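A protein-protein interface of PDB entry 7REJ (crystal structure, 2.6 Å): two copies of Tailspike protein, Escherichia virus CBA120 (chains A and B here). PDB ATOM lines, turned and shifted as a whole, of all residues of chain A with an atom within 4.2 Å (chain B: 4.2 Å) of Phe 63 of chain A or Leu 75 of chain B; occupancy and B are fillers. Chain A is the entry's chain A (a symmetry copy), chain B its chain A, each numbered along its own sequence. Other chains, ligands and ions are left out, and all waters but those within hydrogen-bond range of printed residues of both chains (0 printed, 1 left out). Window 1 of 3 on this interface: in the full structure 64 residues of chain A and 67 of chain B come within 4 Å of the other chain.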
ATOM      1  N   ARG A  55       0.307  -4.271  -9.226  1.00  0.00           N
ATOM      2  CA  ARG A  55      -0.715  -5.042  -8.453  1.00  0.00           C
ATOM      3  C   ARG A  55      -0.688  -4.727  -6.969  1.00  0.00           C
ATOM      4  O   ARG A  55       0.278  -4.170  -6.483  1.00  0.00           O
ATOM      5  CB  ARG A  55      -0.608  -6.565  -8.629  1.00  0.00           C
ATOM      6  CG  ARG A  55       0.228  -7.331  -7.610  1.00  0.00           C
ATOM      7  CD  ARG A  55       0.731  -8.580  -8.324  1.00  0.00           C
ATOM      8  NE  ARG A  55       1.376  -9.615  -7.521  1.00  0.00           N
ATOM      9  CZ  ARG A  55       1.750 -10.815  -7.982  1.00  0.00           C
ATOM     10  NH1 ARG A  55       2.327 -11.681  -7.169  1.00  0.00           N
ATOM     11  NH2 ARG A  55       1.550 -11.155  -9.245  1.00  0.00           N
ATOM     12  N   TYR A  56      -1.766  -5.105  -6.303  1.00  0.00           N
ATOM     13  CA  TYR A  56      -1.824  -5.225  -4.833  1.00  0.00           C
ATOM     14  C   TYR A  56      -1.795  -6.725  -4.512  1.00  0.00           C
ATOM     15  O   TYR A  56      -2.694  -7.447  -5.019  1.00  0.00           O
ATOM     16  CB  TYR A  56      -3.033  -4.487  -4.265  1.00  0.00           C
ATOM     17  CG  TYR A  56      -3.339  -4.939  -2.870  1.00  0.00           C
ATOM     18  CD1 TYR A  56      -4.175  -6.018  -2.654  1.00  0.00           C
ATOM     19  CD2 TYR A  56      -2.802  -4.302  -1.768  1.00  0.00           C
ATOM     20  CE1 TYR A  56      -4.478  -6.461  -1.380  1.00  0.00           C
ATOM     21  CE2 TYR A  56      -3.092  -4.730  -0.484  1.00  0.00           C
ATOM     22  CZ  TYR A  56      -3.933  -5.813  -0.289  1.00  0.00           C
ATOM     23  OH  TYR A  56      -4.223  -6.239   0.972  1.00  0.00           O
ATOM     24  N   GLU A  62       1.392  -6.131   0.164  1.00  0.00           N
ATOM     25  CA  GLU A  62       2.368  -5.203  -0.463  1.00  0.00           C
ATOM     26  C   GLU A  62       1.920  -4.854  -1.885  1.00  0.00           C
ATOM     27  O   GLU A  62       1.507  -5.772  -2.666  1.00  0.00           O
ATOM     28  CB  GLU A  62       3.779  -5.789  -0.488  1.00  0.00           C
ATOM     29  CG  GLU A  62       4.695  -5.225   0.599  1.00  0.00           C
ATOM     30  CD  GLU A  62       5.197  -3.801   0.370  1.00  0.00           C
ATOM     31  OE1 GLU A  62       5.432  -3.066   1.372  1.00  0.00           O
ATOM     32  OE2 GLU A  62       5.356  -3.420  -0.823  1.00  0.00           O
ATOM     33  N   PHE A  63       2.003  -3.554  -2.196  1.00  0.00           N
ATOM     34  CA  PHE A  63       1.818  -2.999  -3.569  1.00  0.00           C
ATOM     35  C   PHE A  63       3.074  -3.277  -4.401  1.00  0.00           C
ATOM     36  O   PHE A  63       4.132  -2.605  -4.237  1.00  0.00           O
ATOM     37  CB  PHE A  63       1.514  -1.501  -3.553  1.00  0.00           C
ATOM     38  CG  PHE A  63       0.219  -1.145  -2.879  1.00  0.00           C
ATOM     39  CD1 PHE A  63      -0.978  -1.227  -3.557  1.00  0.00           C
ATOM     40  CD2 PHE A  63       0.195  -0.730  -1.568  1.00  0.00           C
ATOM     41  CE1 PHE A  63      -2.169  -0.898  -2.930  1.00  0.00           C
ATOM     42  CE2 PHE A  63      -0.995  -0.400  -0.940  1.00  0.00           C
ATOM     43  CZ  PHE A  63      -2.178  -0.485  -1.620  1.00  0.00           C
ATOM     44  N   GLU A  64       2.955  -4.263  -5.282  1.00  0.00           N
ATOM     45  CA  GLU A  64       4.083  -4.733  -6.122  1.00  0.00           C
ATOM     46  C   GLU A  64       3.887  -4.151  -7.515  1.00  0.00           C
ATOM     47  O   GLU A  64       2.747  -4.069  -7.907  1.00  0.00           O
ATOM     48  CB  GLU A  64       4.125  -6.260  -6.175  1.00  0.00           C
ATOM     49  CG  GLU A  64       3.669  -6.919  -4.889  1.00  0.00           C
ATOM     50  CD  GLU A  64       4.070  -8.383  -4.796  1.00  0.00           C
ATOM     51  OE1 GLU A  64       3.559  -9.160  -5.657  1.00  0.00           O
ATOM     52  OE2 GLU A  64       4.900  -8.757  -3.858  1.00  0.00           O
ATOM     53  N   SER A  74       8.343  -4.848  -4.783  1.00  0.00           N
ATOM     54  CA  SER A  74       7.661  -3.713  -4.109  1.00  0.00           C
ATOM     55  C   SER A  74       7.910  -2.456  -4.931  1.00  0.00           C
ATOM     56  O   SER A  74       8.956  -2.428  -5.602  1.00  0.00           O
ATOM     57  CB  SER A  74       8.133  -3.550  -2.685  1.00  0.00           C
ATOM     58  OG  SER A  74       7.517  -4.492  -1.820  1.00  0.00           O
ATOM     59  N   LEU A  75       7.004  -1.484  -4.880  1.00  0.00           N
ATOM     60  CA  LEU A  75       7.085  -0.330  -5.805  1.00  0.00           C
ATOM     61  C   LEU A  75       8.109   0.687  -5.291  1.00  0.00           C
ATOM     62  O   LEU A  75       8.104   0.985  -4.063  1.00  0.00           O
ATOM     63  CB  LEU A  75       5.717   0.313  -5.945  1.00  0.00           C
ATOM     64  CG  LEU A  75       4.652  -0.529  -6.639  1.00  0.00           C
ATOM     65  CD1 LEU A  75       3.285   0.059  -6.352  1.00  0.00           C
ATOM     66  CD2 LEU A  75       4.883  -0.605  -8.145  1.00  0.00           C
ATOM     67  N   SER B  52      -5.883  -1.998  -1.404  1.00  0.00           N
ATOM     68  CA  SER B  52      -5.467  -1.825  -2.817  1.00  0.00           C
ATOM     69  C   SER B  52      -5.821  -0.435  -3.324  1.00  0.00           C
ATOM     70  O   SER B  52      -5.376  -0.128  -4.452  1.00  0.00           O
ATOM     71  CB  SER B  52      -5.981  -2.869  -3.738  1.00  0.00           C
ATOM     72  OG  SER B  52      -7.369  -2.696  -3.906  1.00  0.00           O
ATOM     73  N   SER B  53      -6.565   0.362  -2.559  1.00  0.00           N
ATOM     74  CA  SER B  53      -6.872   1.752  -2.995  1.00  0.00           C
ATOM     75  C   SER B  53      -5.541   2.496  -3.080  1.00  0.00           C
ATOM     76  O   SER B  53      -4.776   2.363  -2.148  1.00  0.00           O
ATOM     77  CB  SER B  53      -7.804   2.509  -2.072  1.00  0.00           C
ATOM     78  OG  SER B  53      -8.870   1.714  -1.546  1.00  0.00           O
ATOM     79  N   VAL B  54      -5.244   3.251  -4.126  1.00  0.00           N
ATOM     80  CA  VAL B  54      -3.953   4.004  -4.144  1.00  0.00           C
ATOM     81  C   VAL B  54      -4.267   5.489  -4.292  1.00  0.00           C
ATOM     82  O   VAL B  54      -5.344   5.815  -4.862  1.00  0.00           O
ATOM     83  CB  VAL B  54      -3.004   3.498  -5.239  1.00  0.00           C
ATOM     84  CG1 VAL B  54      -3.238   2.042  -5.519  1.00  0.00           C
ATOM     85  CG2 VAL B  54      -3.134   4.306  -6.506  1.00  0.00           C
ATOM     86  N   PHE B  63       3.048   9.575  -2.703  1.00  0.00           N
ATOM     87  CA  PHE B  63       2.194   8.514  -3.318  1.00  0.00           C
ATOM     88  C   PHE B  63       1.972   7.390  -2.302  1.00  0.00           C
ATOM     89  O   PHE B  63       2.882   6.551  -2.043  1.00  0.00           O
ATOM     90  CB  PHE B  63       2.800   7.955  -4.606  1.00  0.00           C
ATOM     91  CG  PHE B  63       2.921   8.962  -5.714  1.00  0.00           C
ATOM     92  CD1 PHE B  63       1.848   9.255  -6.527  1.00  0.00           C
ATOM     93  CD2 PHE B  63       4.109   9.618  -5.946  1.00  0.00           C
ATOM     94  CE1 PHE B  63       1.967  10.183  -7.547  1.00  0.00           C
ATOM     95  CE2 PHE B  63       4.229  10.547  -6.966  1.00  0.00           C
ATOM     96  CZ  PHE B  63       3.158  10.831  -7.767  1.00  0.00           C
ATOM     97  N   GLU B  64       0.774   7.379  -1.732  1.00  0.00           N
ATOM     98  CA  GLU B  64       0.398   6.418  -0.666  1.00  0.00           C
ATOM     99  C   GLU B  64      -0.463   5.340  -1.309  1.00  0.00           C
ATOM    100  O   GLU B  64      -1.216   5.704  -2.181  1.00  0.00           O
ATOM    101  CB  GLU B  64      -0.364   7.119   0.457  1.00  0.00           C
ATOM    102  CG  GLU B  64       0.096   8.542   0.698  1.00  0.00           C
ATOM    103  CD  GLU B  64      -0.370   9.100   2.035  1.00  0.00           C
ATOM    104  OE1 GLU B  64      -1.621   9.225   2.186  1.00  0.00           O
ATOM    105  OE2 GLU B  64       0.522   9.414   2.937  1.00  0.00           O
ATOM    106  N   GLY B  65      -0.345   4.082  -0.885  1.00  0.00           N
ATOM    107  CA  GLY B  65      -1.368   3.026  -1.038  1.00  0.00           C
ATOM    108  C   GLY B  65      -1.983   2.730   0.315  1.00  0.00           C
ATOM    109  O   GLY B  65      -1.362   3.102   1.358  1.00  0.00           O
ATOM    110  N   TYR B  66      -3.144   2.095   0.337  1.00  0.00           N
ATOM    111  CA  TYR B  66      -3.876   1.814   1.599  1.00  0.00           C
ATOM    112  C   TYR B  66      -3.722   0.336   1.941  1.00  0.00           C
ATOM    113  O   TYR B  66      -4.414  -0.513   1.325  1.00  0.00           O
ATOM    114  CB  TYR B  66      -5.335   2.244   1.525  1.00  0.00           C
ATOM    115  CG  TYR B  66      -6.163   2.039   2.770  1.00  0.00           C
ATOM    116  CD1 TYR B  66      -6.640   0.781   3.126  1.00  0.00           C
ATOM    117  CD2 TYR B  66      -6.481   3.098   3.604  1.00  0.00           C
ATOM    118  CE1 TYR B  66      -7.405   0.578   4.270  1.00  0.00           C
ATOM    119  CE2 TYR B  66      -7.245   2.910   4.752  1.00  0.00           C
ATOM    120  CZ  TYR B  66      -7.712   1.649   5.092  1.00  0.00           C
ATOM    121  OH  TYR B  66      -8.464   1.464   6.221  1.00  0.00           O
ATOM    122  N   TYR B  67      -2.832   0.054   2.904  1.00  0.00           N
ATOM    123  CA  TYR B  67      -2.436  -1.322   3.304  1.00  0.00           C
ATOM    124  C   TYR B  67      -3.405  -1.815   4.375  1.00  0.00           C
ATOM    125  O   TYR B  67      -3.766  -0.999   5.248  1.00  0.00           O
ATOM    126  CB  TYR B  67      -1.004  -1.374   3.826  1.00  0.00           C
ATOM    127  CG  TYR B  67       0.093  -0.946   2.880  1.00  0.00           C
ATOM    128  CD1 TYR B  67       0.289   0.393   2.559  1.00  0.00           C
ATOM    129  CD2 TYR B  67       0.939  -1.883   2.302  1.00  0.00           C
ATOM    130  CE1 TYR B  67       1.296   0.791   1.690  1.00  0.00           C
ATOM    131  CE2 TYR B  67       1.950  -1.505   1.432  1.00  0.00           C
ATOM    132  CZ  TYR B  67       2.127  -0.163   1.127  1.00  0.00           C
ATOM    133  OH  TYR B  67       3.107   0.246   0.278  1.00  0.00           O
ATOM    134  N   LEU B  73      -0.206   4.402   3.609  1.00  0.00           N
ATOM    135  CA  LEU B  73       1.262   4.341   3.805  1.00  0.00           C
ATOM    136  C   LEU B  73       1.931   4.557   2.449  1.00  0.00           C
ATOM    137  O   LEU B  73       1.260   4.420   1.432  1.00  0.00           O
ATOM    138  CB  LEU B  73       1.651   2.985   4.412  1.00  0.00           C
ATOM    139  N   SER B  74       3.208   4.883   2.448  1.00  0.00           N
ATOM    140  CA  SER B  74       3.975   5.148   1.203  1.00  0.00           C
ATOM    141  C   SER B  74       4.067   3.847   0.419  1.00  0.00           C
ATOM    142  O   SER B  74       4.025   2.795   1.079  1.00  0.00           O
ATOM    143  CB  SER B  74       5.340   5.716   1.503  1.00  0.00           C
ATOM    144  OG  SER B  74       5.272   7.101   1.809  1.00  0.00           O
ATOM    145  N   LEU B  75       4.183   3.919  -0.904  1.00  0.00           N
ATOM    146  CA  LEU B  75       4.075   2.698  -1.737  1.00  0.00           C
ATOM    147  C   LEU B  75       5.403   1.934  -1.729  1.00  0.00           C
ATOM    148  O   LEU B  75       6.477   2.584  -1.867  1.00  0.00           O
ATOM    149  CB  LEU B  75       3.687   3.078  -3.154  1.00  0.00           C
ATOM    150  CG  LEU B  75       2.289   3.662  -3.329  1.00  0.00           C
ATOM    151  CD1 LEU B  75       2.199   4.344  -4.680  1.00  0.00           C
ATOM    152  CD2 LEU B  75       1.210   2.591  -3.212  1.00  0.00           C
ATOM    153  N   GLY B  76       5.312   0.605  -1.571  1.00  0.00           N
ATOM    154  CA  GLY B  76       6.463  -0.267  -1.258  1.00  0.00           C
ATOM    155  C   GLY B  76       7.250   0.318  -0.093  1.00  0.00           C
ATOM    156  O   GLY B  76       8.330   0.901  -0.354  1.00  0.00           O
ATOM    157  N   GLY B  77       6.733   0.171   1.140  1.00  0.00           N
ATOM    158  CA  GLY B  77       7.300   0.821   2.346  1.00  0.00           C
ATOM    159  C   GLY B  77       7.677   2.275   2.063  1.00  0.00           C
ATOM    160  O   GLY B  77       6.800   2.996   1.555  1.00  0.00           O
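Of the 13 printed residues of chain B, 8 touch a printed residue of chain A.
Of the 7 printed residues of chain A, 5 touch a printed residue of chain B.
Printed residues of chain A that touch a printed residue of chain B: Tyr 56, Glu 62, Phe 63, Ser 74 and Leu 75.
Among the printed residues, no Asp or Glu carboxylate lies within 4 Å of a Lys or Arg side-chain nitrogen of the other chain.
Phe 63 of chain A touches Leu 75 of chain B, but with the chains exchanged Leu 75 of chain A does not touch Phe 63 of chain B (7.8 Å).
Leu 75 of chain A touches its own counterpart, Leu 75 of chain B.
4 positions are printed for both chains.
Of the 13 pairs that touch across the chains among the printed residues, 1 has its exchanged pair printed and touching as well.
The side-chain carboxylate (OE1) of Glu 62 of chain A sits at hydrogen-bond distance from the backbone NH (N) of Gly 77 of chain B (3.5 Å).
The backbone carbonyl oxygen (O) of Leu 75 of chain A sits close to the backbone carbonyl oxygen (O) of Leu 75 of chain B (3.2 Å).
Tyr 56 of chain A touches Ser 52 of chain B.
OE1 of Glu 62 of chain A touches CE2 of Tyr 67 of chain B, 3.8 Å away.
Gly 76 of chain B touches Glu 62 of chain A (CA to OE2, 3.4 Å).
Phe 63 of chain A touches Ser 52 of chain B (CE1 to CA, 3.4 Å).
Phe 63 of chain A touches Ser 53 of chain B.
Phe 63 of chain A touches Gly 65 of chain B (CE2 to CA, 3.4 Å).
CZ of Phe 63 of chain A touches N of Tyr 66 of chain B, at 3.4 Å.
Tyr 67 of chain B touches Phe 63 of chain A.
Ser 74 of chain A touches Gly 76 of chain B (CB to CA, 3.95 Å).
Leu 75 of chain A touches Gly 76 of chain B.
Phe 63 of chain A touches just these residues of chain B: Ser 52, Ser 53, Gly 65, Tyr 66, Tyr 67 and Leu 75.
Phe 63 of chain B touches none of the printed residues of chain A.
Glu 64 of chain B touches none of the printed residues of chain A.
Of the printed residues of chain A, Tyr 66 of chain B touches Phe 63.
Leu 75 of chain B touches just these residues of chain A: Phe 63 (3.8 Å) and Leu 75 (3.2 Å).
Of the printed residues of chain A, Gly 77 of chain B touches Glu 62 (3.5 Å).
The nearest residue of chain B that does not touch Phe 63 of chain A is Val 54 of chain B (4.1 Å).
N of Gly 65 of chain B sits at hydrogen-bond distance from O of Leu 73 of chain B, 2.8 Å away.
The backbone carbonyl oxygen of Ser 53 of chain B lies within hydrogen-bond range of the backbone NH of Tyr 66 of chain B (3.0 Å).
OE2 of Glu 62 of chain A is in hydrogen-bond range of OG of Ser 74 of chain A, 2.6 Å away.
The backbone NH (N) of Ser 52 of chain B is in hydrogen-bond range of the backbone carbonyl oxygen (O) of Tyr 66 of chain B, at 3.4 Å.
OH of Tyr 67 of chain B is in hydrogen-bond range of O of Ser 74 of chain B.
N of Leu 75 of chain B sits at hydrogen-bond distance from O of Phe 63 of chain B, 3.1 Å away.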
